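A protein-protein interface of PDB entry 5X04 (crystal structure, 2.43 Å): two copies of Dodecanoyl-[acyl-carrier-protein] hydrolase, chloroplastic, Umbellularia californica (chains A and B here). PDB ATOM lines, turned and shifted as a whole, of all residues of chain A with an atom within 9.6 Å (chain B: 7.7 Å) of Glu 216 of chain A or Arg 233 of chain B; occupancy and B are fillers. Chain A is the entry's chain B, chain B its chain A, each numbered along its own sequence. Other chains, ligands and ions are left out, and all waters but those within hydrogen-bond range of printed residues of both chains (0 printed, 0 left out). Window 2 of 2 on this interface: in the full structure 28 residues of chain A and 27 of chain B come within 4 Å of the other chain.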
ATOM      1  N   PRO A  31      -7.443   3.652 -19.055  1.00  0.00           N
ATOM      2  CA  PRO A  31      -8.768   3.033 -19.179  1.00  0.00           C
ATOM      3  C   PRO A  31      -9.031   1.990 -18.092  1.00  0.00           C
ATOM      4  O   PRO A  31     -10.185   1.665 -17.813  1.00  0.00           O
ATOM      5  CB  PRO A  31      -8.723   2.372 -20.562  1.00  0.00           C
ATOM      6  CG  PRO A  31      -7.647   3.097 -21.301  1.00  0.00           C
ATOM      7  CD  PRO A  31      -6.629   3.467 -20.268  1.00  0.00           C
ATOM      8  N   ASP A  32      -7.961   1.480 -17.491  1.00  0.00           N
ATOM      9  CA  ASP A  32      -8.061   0.524 -16.394  1.00  0.00           C
ATOM     10  C   ASP A  32      -8.134   1.243 -15.055  1.00  0.00           C
ATOM     11  O   ASP A  32      -8.028   0.614 -13.998  1.00  0.00           O
ATOM     12  CB  ASP A  32      -6.868  -0.437 -16.408  1.00  0.00           C
ATOM     13  CG  ASP A  32      -5.529   0.286 -16.414  1.00  0.00           C
ATOM     14  OD1 ASP A  32      -5.500   1.516 -16.191  1.00  0.00           O
ATOM     15  OD2 ASP A  32      -4.496  -0.379 -16.637  1.00  0.00           O
ATOM     16  N   SER A  34      -5.976   2.962 -13.751  1.00  0.00           N
ATOM     17  CA  SER A  34      -4.649   3.076 -13.156  1.00  0.00           C
ATOM     18  C   SER A  34      -3.856   4.258 -13.715  1.00  0.00           C
ATOM     19  O   SER A  34      -3.859   4.511 -14.922  1.00  0.00           O
ATOM     20  CB  SER A  34      -3.862   1.781 -13.360  1.00  0.00           C
ATOM     21  OG  SER A  34      -4.208   0.824 -12.375  1.00  0.00           O
ATOM     22  N   VAL A 210       6.259  -1.005 -27.455  1.00  0.00           N
ATOM     23  CA  VAL A 210       5.615  -1.960 -26.569  1.00  0.00           C
ATOM     24  C   VAL A 210       4.191  -2.141 -27.070  1.00  0.00           C
ATOM     25  O   VAL A 210       3.430  -1.175 -27.138  1.00  0.00           O
ATOM     26  CB  VAL A 210       5.615  -1.498 -25.101  1.00  0.00           C
ATOM     27  CG1 VAL A 210       4.780  -2.444 -24.247  1.00  0.00           C
ATOM     28  CG2 VAL A 210       7.038  -1.414 -24.572  1.00  0.00           C
ATOM     29  N   PRO A 211       3.822  -3.380 -27.424  1.00  0.00           N
ATOM     30  CA  PRO A 211       2.497  -3.643 -27.989  1.00  0.00           C
ATOM     31  C   PRO A 211       1.400  -3.401 -26.964  1.00  0.00           C
ATOM     32  O   PRO A 211       1.621  -3.632 -25.775  1.00  0.00           O
ATOM     33  CB  PRO A 211       2.575  -5.119 -28.387  1.00  0.00           C
ATOM     34  CG  PRO A 211       3.572  -5.698 -27.447  1.00  0.00           C
ATOM     35  CD  PRO A 211       4.599  -4.617 -27.241  1.00  0.00           C
ATOM     36  N   ASP A 212       0.247  -2.921 -27.420  1.00  0.00           N
ATOM     37  CA  ASP A 212      -0.882  -2.637 -26.540  1.00  0.00           C
ATOM     38  C   ASP A 212      -1.249  -3.832 -25.665  1.00  0.00           C
ATOM     39  O   ASP A 212      -1.734  -3.661 -24.549  1.00  0.00           O
ATOM     40  CB  ASP A 212      -2.103  -2.207 -27.361  1.00  0.00           C
ATOM     41  CG  ASP A 212      -1.998  -0.781 -27.863  1.00  0.00           C
ATOM     42  OD1 ASP A 212      -1.056  -0.071 -27.452  1.00  0.00           O
ATOM     43  OD2 ASP A 212      -2.859  -0.370 -28.668  1.00  0.00           O
ATOM     44  N   SER A 213      -0.984  -5.036 -26.165  1.00  0.00           N
ATOM     45  CA  SER A 213      -1.327  -6.269 -25.461  1.00  0.00           C
ATOM     46  C   SER A 213      -0.655  -6.400 -24.093  1.00  0.00           C
ATOM     47  O   SER A 213      -1.201  -7.031 -23.188  1.00  0.00           O
ATOM     48  CB  SER A 213      -0.957  -7.478 -26.323  1.00  0.00           C
ATOM     49  OG  SER A 213       0.330  -7.319 -26.895  1.00  0.00           O
ATOM     50  N   ILE A 214       0.524  -5.806 -23.944  1.00  0.00           N
ATOM     51  CA  ILE A 214       1.246  -5.865 -22.678  1.00  0.00           C
ATOM     52  C   ILE A 214       0.704  -4.827 -21.694  1.00  0.00           C
ATOM     53  O   ILE A 214       0.604  -5.086 -20.493  1.00  0.00           O
ATOM     54  CB  ILE A 214       2.759  -5.649 -22.892  1.00  0.00           C
ATOM     55  CG1 ILE A 214       3.330  -6.769 -23.765  1.00  0.00           C
ATOM     56  CG2 ILE A 214       3.492  -5.571 -21.559  1.00  0.00           C
ATOM     57  CD1 ILE A 214       4.837  -6.766 -23.863  1.00  0.00           C
ATOM     58  N   PHE A 215       0.338  -3.661 -22.216  1.00  0.00           N
ATOM     59  CA  PHE A 215      -0.269  -2.611 -21.406  1.00  0.00           C
ATOM     60  C   PHE A 215      -1.630  -3.048 -20.878  1.00  0.00           C
ATOM     61  O   PHE A 215      -2.044  -2.652 -19.790  1.00  0.00           O
ATOM     62  CB  PHE A 215      -0.419  -1.323 -22.216  1.00  0.00           C
ATOM     63  CG  PHE A 215       0.863  -0.563 -22.392  1.00  0.00           C
ATOM     64  CD1 PHE A 215       1.524  -0.029 -21.299  1.00  0.00           C
ATOM     65  CD2 PHE A 215       1.402  -0.376 -23.653  1.00  0.00           C
ATOM     66  CE1 PHE A 215       2.704   0.673 -21.462  1.00  0.00           C
ATOM     67  CE2 PHE A 215       2.579   0.325 -23.824  1.00  0.00           C
ATOM     68  CZ  PHE A 215       3.230   0.850 -22.726  1.00  0.00           C
ATOM     69  N   GLU A 216      -2.319  -3.866 -21.666  1.00  0.00           N
ATOM     70  CA  GLU A 216      -3.638  -4.369 -21.305  1.00  0.00           C
ATOM     71  C   GLU A 216      -3.552  -5.437 -20.218  1.00  0.00           C
ATOM     72  O   GLU A 216      -4.403  -5.504 -19.332  1.00  0.00           O
ATOM     73  CB  GLU A 216      -4.340  -4.933 -22.542  1.00  0.00           C
ATOM     74  CG  GLU A 216      -4.621  -3.895 -23.617  1.00  0.00           C
ATOM     75  CD  GLU A 216      -5.678  -4.337 -24.607  1.00  0.00           C
ATOM     76  OE1 GLU A 216      -6.517  -5.188 -24.248  1.00  0.00           O
ATOM     77  OE2 GLU A 216      -5.657  -3.842 -25.754  1.00  0.00           O
ATOM     78  N   SER A 217      -2.519  -6.269 -20.295  1.00  0.00           N
ATOM     79  CA  SER A 217      -2.386  -7.413 -19.398  1.00  0.00           C
ATOM     80  C   SER A 217      -1.587  -7.108 -18.129  1.00  0.00           C
ATOM     81  O   SER A 217      -1.887  -7.642 -17.061  1.00  0.00           O
ATOM     82  CB  SER A 217      -1.734  -8.583 -20.140  1.00  0.00           C
ATOM     83  OG  SER A 217      -0.542  -8.172 -20.789  1.00  0.00           O
ATOM     84  N   HIS A 218      -0.575  -6.254 -18.246  1.00  0.00           N
ATOM     85  CA  HIS A 218       0.380  -6.056 -17.158  1.00  0.00           C
ATOM     86  C   HIS A 218       0.567  -4.602 -16.724  1.00  0.00           C
ATOM     87  O   HIS A 218       0.295  -3.669 -17.481  1.00  0.00           O
ATOM     88  CB  HIS A 218       1.747  -6.628 -17.551  1.00  0.00           C
ATOM     89  CG  HIS A 218       1.803  -8.123 -17.561  1.00  0.00           C
ATOM     90  ND1 HIS A 218       1.129  -8.890 -18.486  1.00  0.00           N
ATOM     91  CD2 HIS A 218       2.472  -8.994 -16.767  1.00  0.00           C
ATOM     92  CE1 HIS A 218       1.370 -10.168 -18.255  1.00  0.00           C
ATOM     93  NE2 HIS A 218       2.182 -10.258 -17.217  1.00  0.00           N
ATOM     94  N   HIS A 219       1.036  -4.433 -15.491  1.00  0.00           N
ATOM     95  CA  HIS A 219       1.499  -3.145 -14.980  1.00  0.00           C
ATOM     96  C   HIS A 219       3.020  -3.152 -14.892  1.00  0.00           C
ATOM     97  O   HIS A 219       3.619  -4.171 -14.550  1.00  0.00           O
ATOM     98  CB  HIS A 219       0.904  -2.845 -13.601  1.00  0.00           C
ATOM     99  CG  HIS A 219      -0.491  -2.305 -13.639  1.00  0.00           C
ATOM    100  ND1 HIS A 219      -1.419  -2.577 -12.656  1.00  0.00           N
ATOM    101  CD2 HIS A 219      -1.109  -1.491 -14.526  1.00  0.00           C
ATOM    102  CE1 HIS A 219      -2.554  -1.963 -12.943  1.00  0.00           C
ATOM    103  NE2 HIS A 219      -2.391  -1.297 -14.073  1.00  0.00           N
ATOM    104  N   ILE A 220       3.648  -2.022 -15.201  1.00  0.00           N
ATOM    105  CA  ILE A 220       5.087  -1.892 -15.006  1.00  0.00           C
ATOM    106  C   ILE A 220       5.420  -1.896 -13.519  1.00  0.00           C
ATOM    107  O   ILE A 220       4.881  -1.099 -12.753  1.00  0.00           O
ATOM    108  CB  ILE A 220       5.646  -0.605 -15.641  1.00  0.00           C
ATOM    109  CG1 ILE A 220       5.511  -0.655 -17.161  1.00  0.00           C
ATOM    110  CG2 ILE A 220       7.105  -0.417 -15.261  1.00  0.00           C
ATOM    111  CD1 ILE A 220       5.774   0.669 -17.841  1.00  0.00           C
ATOM    112  N   TRP A 273       7.495  -6.435 -15.655  1.00  0.00           N
ATOM    113  CA  TRP A 273       6.041  -6.353 -15.577  1.00  0.00           C
ATOM    114  C   TRP A 273       5.439  -7.417 -14.677  1.00  0.00           C
ATOM    115  O   TRP A 273       5.989  -8.507 -14.513  1.00  0.00           O
ATOM    116  CB  TRP A 273       5.425  -6.468 -16.973  1.00  0.00           C
ATOM    117  CG  TRP A 273       5.906  -5.433 -17.928  1.00  0.00           C
ATOM    118  CD1 TRP A 273       7.155  -5.331 -18.446  1.00  0.00           C
ATOM    119  CD2 TRP A 273       5.140  -4.374 -18.521  1.00  0.00           C
ATOM    120  NE1 TRP A 273       7.230  -4.264 -19.306  1.00  0.00           N
ATOM    121  CE2 TRP A 273       6.002  -3.661 -19.372  1.00  0.00           C
ATOM    122  CE3 TRP A 273       3.809  -3.957 -18.403  1.00  0.00           C
ATOM    123  CZ2 TRP A 273       5.582  -2.554 -20.107  1.00  0.00           C
ATOM    124  CZ3 TRP A 273       3.394  -2.857 -19.134  1.00  0.00           C
ATOM    125  CH2 TRP A 273       4.277  -2.169 -19.975  1.00  0.00           C
ATOM    126  N   ARG A 274       4.295  -7.080 -14.097  1.00  0.00           N
ATOM    127  CA  ARG A 274       3.511  -8.011 -13.306  1.00  0.00           C
ATOM    128  C   ARG A 274       2.063  -7.985 -13.783  1.00  0.00           C
ATOM    129  O   ARG A 274       1.567  -6.938 -14.200  1.00  0.00           O
ATOM    130  CB  ARG A 274       3.606  -7.658 -11.822  1.00  0.00           C
ATOM    131  CG  ARG A 274       3.125  -6.252 -11.506  1.00  0.00           C
ATOM    132  CD  ARG A 274       3.005  -6.006 -10.014  1.00  0.00           C
ATOM    133  NE  ARG A 274       2.800  -4.590  -9.725  1.00  0.00           N
ATOM    134  CZ  ARG A 274       1.636  -3.959  -9.845  1.00  0.00           C
ATOM    135  NH1 ARG A 274       0.560  -4.616 -10.255  1.00  0.00           N
ATOM    136  NH2 ARG A 274       1.550  -2.667  -9.560  1.00  0.00           N
ATOM    137  N   PRO A 275       1.387  -9.143 -13.741  1.00  0.00           N
ATOM    138  CA  PRO A 275      -0.028  -9.214 -14.118  1.00  0.00           C
ATOM    139  C   PRO A 275      -0.894  -8.322 -13.233  1.00  0.00           C
ATOM    140  O   PRO A 275      -0.664  -8.242 -12.026  1.00  0.00           O
ATOM    141  CB  PRO A 275      -0.375 -10.696 -13.924  1.00  0.00           C
ATOM    142  CG  PRO A 275       0.703 -11.241 -13.043  1.00  0.00           C
ATOM    143  CD  PRO A 275       1.930 -10.463 -13.385  1.00  0.00           C
ATOM    144  N   LYS A 276      -1.871  -7.657 -13.839  1.00  0.00           N
ATOM    145  CA  LYS A 276      -2.706  -6.694 -13.132  1.00  0.00           C
ATOM    146  C   LYS A 276      -3.568  -7.363 -12.065  1.00  0.00           C
ATOM    147  O   LYS A 276      -4.556  -8.027 -12.376  1.00  0.00           O
ATOM    148  CB  LYS A 276      -3.590  -5.939 -14.125  1.00  0.00           C
ATOM    149  CG  LYS A 276      -2.823  -4.959 -14.997  1.00  0.00           C
ATOM    150  CD  LYS A 276      -3.743  -4.196 -15.931  1.00  0.00           C
ATOM    151  CE  LYS A 276      -2.951  -3.238 -16.804  1.00  0.00           C
ATOM    152  NZ  LYS A 276      -3.779  -2.650 -17.892  1.00  0.00           N
ATOM    153  N   THR B 185      -3.445   6.705 -35.679  1.00  0.00           N
ATOM    154  CA  THR B 185      -4.230   5.644 -35.066  1.00  0.00           C
ATOM    155  C   THR B 185      -4.155   5.733 -33.544  1.00  0.00           C
ATOM    156  O   THR B 185      -3.114   6.075 -32.982  1.00  0.00           O
ATOM    157  CB  THR B 185      -3.765   4.245 -35.550  1.00  0.00           C
ATOM    158  OG1 THR B 185      -4.725   3.255 -35.158  1.00  0.00           O
ATOM    159  CG2 THR B 185      -2.400   3.881 -34.982  1.00  0.00           C
ATOM    160  N   PRO B 186      -5.281   5.467 -32.869  1.00  0.00           N
ATOM    161  CA  PRO B 186      -5.282   5.544 -31.409  1.00  0.00           C
ATOM    162  C   PRO B 186      -4.696   4.284 -30.790  1.00  0.00           C
ATOM    163  O   PRO B 186      -4.828   3.199 -31.356  1.00  0.00           O
ATOM    164  CB  PRO B 186      -6.766   5.682 -31.073  1.00  0.00           C
ATOM    165  CG  PRO B 186      -7.448   4.929 -32.163  1.00  0.00           C
ATOM    166  CD  PRO B 186      -6.619   5.157 -33.405  1.00  0.00           C
ATOM    167  N   ARG B 187      -4.050   4.431 -29.641  1.00  0.00           N
ATOM    168  CA  ARG B 187      -3.547   3.279 -28.912  1.00  0.00           C
ATOM    169  C   ARG B 187      -4.447   3.005 -27.717  1.00  0.00           C
ATOM    170  O   ARG B 187      -5.388   3.754 -27.455  1.00  0.00           O
ATOM    171  CB  ARG B 187      -2.096   3.487 -28.472  1.00  0.00           C
ATOM    172  CG  ARG B 187      -1.102   3.456 -29.625  1.00  0.00           C
ATOM    173  CD  ARG B 187       0.333   3.404 -29.129  1.00  0.00           C
ATOM    174  NE  ARG B 187       0.522   2.340 -28.148  1.00  0.00           N
ATOM    175  CZ  ARG B 187       1.698   1.797 -27.848  1.00  0.00           C
ATOM    176  NH1 ARG B 187       2.798   2.213 -28.461  1.00  0.00           N
ATOM    177  NH2 ARG B 187       1.773   0.834 -26.940  1.00  0.00           N
ATOM    178  N   TRP B 188      -4.154   1.920 -27.008  1.00  0.00           N
ATOM    179  CA  TRP B 188      -4.987   1.436 -25.913  1.00  0.00           C
ATOM    180  C   TRP B 188      -5.404   2.482 -24.877  1.00  0.00           C
ATOM    181  O   TRP B 188      -6.565   2.525 -24.472  1.00  0.00           O
ATOM    182  CB  TRP B 188      -4.251   0.295 -25.210  1.00  0.00           C
ATOM    183  CG  TRP B 188      -4.745   0.012 -23.837  1.00  0.00           C
ATOM    184  CD1 TRP B 188      -5.863  -0.686 -23.490  1.00  0.00           C
ATOM    185  CD2 TRP B 188      -4.126   0.417 -22.614  1.00  0.00           C
ATOM    186  NE1 TRP B 188      -5.981  -0.737 -22.122  1.00  0.00           N
ATOM    187  CE2 TRP B 188      -4.925  -0.066 -21.561  1.00  0.00           C
ATOM    188  CE3 TRP B 188      -2.972   1.146 -22.306  1.00  0.00           C
ATOM    189  CZ2 TRP B 188      -4.609   0.154 -20.222  1.00  0.00           C
ATOM    190  CZ3 TRP B 188      -2.659   1.363 -20.978  1.00  0.00           C
ATOM    191  CH2 TRP B 188      -3.474   0.870 -19.952  1.00  0.00           C
ATOM    192  N   ASN B 189      -4.471   3.329 -24.455  1.00  0.00           N
ATOM    193  CA  ASN B 189      -4.768   4.323 -23.427  1.00  0.00           C
ATOM    194  C   ASN B 189      -5.479   5.562 -23.978  1.00  0.00           C
ATOM    195  O   ASN B 189      -5.928   6.417 -23.214  1.00  0.00           O
ATOM    196  CB  ASN B 189      -3.490   4.731 -22.689  1.00  0.00           C
ATOM    197  CG  ASN B 189      -2.571   5.581 -23.535  1.00  0.00           C
ATOM    198  OD1 ASN B 189      -2.693   6.806 -23.565  1.00  0.00           O
ATOM    199  ND2 ASN B 189      -1.637   4.937 -24.225  1.00  0.00           N
ATOM    200  N   ASP B 190      -5.581   5.654 -25.301  1.00  0.00           N
ATOM    201  CA  ASP B 190      -6.214   6.805 -25.940  1.00  0.00           C
ATOM    202  C   ASP B 190      -7.737   6.685 -25.985  1.00  0.00           C
ATOM    203  O   ASP B 190      -8.423   7.604 -26.435  1.00  0.00           O
ATOM    204  CB  ASP B 190      -5.679   6.987 -27.363  1.00  0.00           C
ATOM    205  CG  ASP B 190      -4.204   7.337 -27.394  1.00  0.00           C
ATOM    206  OD1 ASP B 190      -3.714   7.955 -26.426  1.00  0.00           O
ATOM    207  OD2 ASP B 190      -3.534   6.997 -28.394  1.00  0.00           O
ATOM    208  N   LEU B 191      -8.259   5.557 -25.515  1.00  0.00           N
ATOM    209  CA  LEU B 191      -9.691   5.279 -25.588  1.00  0.00           C
ATOM    210  C   LEU B 191     -10.392   5.614 -24.273  1.00  0.00           C
ATOM    211  O   LEU B 191      -9.757   5.651 -23.218  1.00  0.00           O
ATOM    212  CB  LEU B 191      -9.934   3.817 -25.960  1.00  0.00           C
ATOM    213  CG  LEU B 191      -9.409   3.384 -27.331  1.00  0.00           C
ATOM    214  CD1 LEU B 191      -9.431   1.871 -27.454  1.00  0.00           C
ATOM    215  CD2 LEU B 191     -10.220   4.028 -28.446  1.00  0.00           C
ATOM    216  N   GLN B 195     -15.362   2.556 -25.553  1.00  0.00           N
ATOM    217  CA  GLN B 195     -14.876   2.165 -26.896  1.00  0.00           C
ATOM    218  C   GLN B 195     -14.370   3.337 -27.726  1.00  0.00           C
ATOM    219  O   GLN B 195     -13.836   3.135 -28.813  1.00  0.00           O
ATOM    220  CB  GLN B 195     -15.954   1.469 -27.745  1.00  0.00           C
ATOM    221  CG  GLN B 195     -16.934   0.555 -27.043  1.00  0.00           C
ATOM    222  CD  GLN B 195     -18.195   0.374 -27.850  1.00  0.00           C
ATOM    223  OE1 GLN B 195     -18.212  -0.278 -28.902  1.00  0.00           O
ATOM    224  NE2 GLN B 195     -19.259   1.009 -27.385  1.00  0.00           N
ATOM    225  N   HIS B 196     -14.486   4.546 -27.196  1.00  0.00           N
ATOM    226  CA  HIS B 196     -14.260   5.743 -27.996  1.00  0.00           C
ATOM    227  C   HIS B 196     -12.964   6.481 -27.673  1.00  0.00           C
ATOM    228  O   HIS B 196     -12.460   6.418 -26.552  1.00  0.00           O
ATOM    229  CB  HIS B 196     -15.452   6.679 -27.833  1.00  0.00           C
ATOM    230  CG  HIS B 196     -16.707   6.150 -28.452  1.00  0.00           C
ATOM    231  ND1 HIS B 196     -17.953   6.678 -28.184  1.00  0.00           N
ATOM    232  CD2 HIS B 196     -16.910   5.122 -29.307  1.00  0.00           C
ATOM    233  CE1 HIS B 196     -18.864   6.013 -28.870  1.00  0.00           C
ATOM    234  NE2 HIS B 196     -18.258   5.061 -29.558  1.00  0.00           N
ATOM    235  N   VAL B 197     -12.441   7.191 -28.667  1.00  0.00           N
ATOM    236  CA  VAL B 197     -11.187   7.919 -28.519  1.00  0.00           C
ATOM    237  C   VAL B 197     -11.369   9.183 -27.675  1.00  0.00           C
ATOM    238  O   VAL B 197     -12.363   9.897 -27.811  1.00  0.00           O
ATOM    239  CB  VAL B 197     -10.600   8.300 -29.897  1.00  0.00           C
ATOM    240  CG1 VAL B 197      -9.393   9.222 -29.748  1.00  0.00           C
ATOM    241  CG2 VAL B 197     -10.229   7.060 -30.686  1.00  0.00           C
ATOM    242  N   CYS B 231     -14.789   8.207 -32.918  1.00  0.00           N
ATOM    243  CA  CYS B 231     -13.833   7.252 -33.473  1.00  0.00           C
ATOM    244  C   CYS B 231     -13.575   6.086 -32.526  1.00  0.00           C
ATOM    245  O   CYS B 231     -13.740   6.206 -31.313  1.00  0.00           O
ATOM    246  CB  CYS B 231     -12.513   7.946 -33.816  1.00  0.00           C
ATOM    247  SG  CYS B 231     -12.570   8.937 -35.327  1.00  0.00           S
ATOM    248  N   THR B 232     -13.175   4.955 -33.098  1.00  0.00           N
ATOM    249  CA  THR B 232     -12.918   3.748 -32.323  1.00  0.00           C
ATOM    250  C   THR B 232     -11.452   3.336 -32.387  1.00  0.00           C
ATOM    251  O   THR B 232     -10.605   4.076 -32.888  1.00  0.00           O
ATOM    252  CB  THR B 232     -13.785   2.573 -32.803  1.00  0.00           C
ATOM    253  OG1 THR B 232     -13.668   2.442 -34.226  1.00  0.00           O
ATOM    254  CG2 THR B 232     -15.242   2.803 -32.435  1.00  0.00           C
ATOM    255  N   ARG B 233     -11.166   2.144 -31.874  1.00  0.00           N
ATOM    256  CA  ARG B 233      -9.802   1.640 -31.772  1.00  0.00           C
ATOM    257  C   ARG B 233      -9.232   1.248 -33.136  1.00  0.00           C
ATOM    258  O   ARG B 233      -8.019   1.224 -33.334  1.00  0.00           O
ATOM    259  CB  ARG B 233      -9.775   0.447 -30.817  1.00  0.00           C
ATOM    260  CG  ARG B 233      -8.402  -0.093 -30.486  1.00  0.00           C
ATOM    261  CD  ARG B 233      -8.525  -1.129 -29.386  1.00  0.00           C
ATOM    262  NE  ARG B 233      -7.297  -1.278 -28.616  1.00  0.00           N
ATOM    263  CZ  ARG B 233      -7.257  -1.750 -27.375  1.00  0.00           C
ATOM    264  NH1 ARG B 233      -8.379  -2.111 -26.765  1.00  0.00           N
ATOM    265  NH2 ARG B 233      -6.100  -1.856 -26.741  1.00  0.00           N
ATOM    266  N   ASP B 234     -10.122   0.958 -34.078  1.00  0.00           N
ATOM    267  CA  ASP B 234      -9.728   0.544 -35.421  1.00  0.00           C
ATOM    268  C   ASP B 234      -9.887   1.680 -36.414  1.00  0.00           C
ATOM    269  O   ASP B 234      -9.998   1.458 -37.619  1.00  0.00           O
ATOM    270  CB  ASP B 234     -10.552  -0.667 -35.861  1.00  0.00           C
ATOM    271  CG  ASP B 234     -10.248  -1.906 -35.044  1.00  0.00           C
ATOM    272  OD1 ASP B 234      -9.272  -1.883 -34.262  1.00  0.00           O
ATOM    273  OD2 ASP B 234     -11.026  -2.880 -35.136  1.00  0.00           O
ATOM    274  N   SER B 235      -9.900   2.904 -35.901  1.00  0.00           N
ATOM    275  CA  SER B 235      -9.965   4.072 -36.759  1.00  0.00           C
ATOM    276  C   SER B 235      -8.553   4.447 -37.182  1.00  0.00           C
ATOM    277  O   SER B 235      -7.606   4.313 -36.408  1.00  0.00           O
ATOM    278  CB  SER B 235     -10.645   5.244 -36.047  1.00  0.00           C
ATOM    279  OG  SER B 235     -11.983   4.930 -35.700  1.00  0.00           O
ATOM    280  N   VAL B 236      -8.418   4.917 -38.414  1.00  0.00           N
ATOM    281  CA  VAL B 236      -7.143   5.409 -38.913  1.00  0.00           C
ATOM    282  C   VAL B 236      -7.413   6.766 -39.537  1.00  0.00           C
ATOM    283  O   VAL B 236      -8.218   6.875 -40.455  1.00  0.00           O
ATOM    284  CB  VAL B 236      -6.505   4.462 -39.947  1.00  0.00           C
ATOM    285  CG1 VAL B 236      -5.140   4.982 -40.362  1.00  0.00           C
ATOM    286  CG2 VAL B 236      -6.384   3.056 -39.379  1.00  0.00           C
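N of Trp 188 of chain B sits at hydrogen-bond distance from OD2 of Asp 212 of chain A (3.1 Å).
The guanidinium group (NE) of Arg 187 of chain B lies within salt-bridge range of the side-chain carboxylate (OD1) of Asp 212 of chain A (3.0 Å).
NH2 of Arg 187 of chain B sits at hydrogen-bond distance from O of Val 210 of chain A, at 2.6 Å.
NH1 of Arg 233 of chain B is in salt-bridge range of OE2 of Glu 216 of chain A (3.4 Å).
The side-chain amino group (NZ) of Lys 276 of chain A lies within salt-bridge range of the side-chain carboxylate (OD2) of Asp 32 of chain A, at 2.7 Å.
A ring nitrogen (NE2) of His 219 of chain A lies within hydrogen-bond range of the side-chain carboxylate of Asp 32 of chain A (3.4 Å).
O of Phe 215 of chain A sits at hydrogen-bond distance from NZ of Lys 276 of chain A (2.6 Å).
O of Ser 217 of chain A sits at hydrogen-bond distance from N of Lys 276 of chain A (3.2 Å).
OD1 of Asn 189 of chain B lies close to OD1 of Asp 190 of chain B (3.2 Å).
The backbone carbonyl oxygen (O) of Glu 216 of chain A sits at hydrogen-bond distance from the side-chain amino group (NZ) of Lys 276 of chain A, 3.3 Å away.
O of Trp 188 of chain B touches CG of Pro 31 of chain A (3.4 Å).
Pro 31 of chain A touches Asn 189 of chain B (CD to CA, 3.8 Å).
Pro 31 of chain A touches Leu 191 of chain B (CG to O, 3.8 Å).
Asp 32 of chain A touches Trp 188 of chain B (OD2 to CZ2, 3.6 Å).
Phe 215 of chain A touches Arg 187 of chain B (CE2 to NH2, 3.3 Å).
Phe 215 of chain A touches Trp 188 of chain B (CB to CE3, 3.6 Å).
Glu 216 of chain A touches Trp 188 of chain B (CG to CD1, 3.4 Å).
Lys 276 of chain A touches Trp 188 of chain B.
Of chain B, only Trp 188 and Arg 233 come within 4 Å of Glu 216 of chain A.
Of chain A, only Glu 216 (2.3 Å) comes within 4 Å of Arg 233 of chain B.
Pro 186 of chain B touches none of the printed residues of chain A.
Asp 234 of chain B touches none of the printed residues of chain A.
No residue of chain A comes within 4 Å of Ser 235 of chain B.
Printed residues of chain A within 4 Å of Leu 191 of chain B: Pro 31 (3.8 Å).
Printed residues of chain A within 4 Å of Asn 189 of chain B: Pro 31 (3.8 Å).
Ile 220 of chain A touches none of the printed residues of chain B.
Val 197 of chain B touches none of the printed residues of chain A.
Hydrophobic or aromatic side chains of chain B within 4 Å of the printed part of chain A: Trp 188.
Along chain B the printed residues that touch a printed residue of chain A span positions 187 to 233.
Of the 18 printed residues of chain A, 7 touch a printed residue of chain B.
No position is printed for both chains.
Of the 12 pairs that touch across the chains among the printed residues, none has its exchanged pair printed and touching as well.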
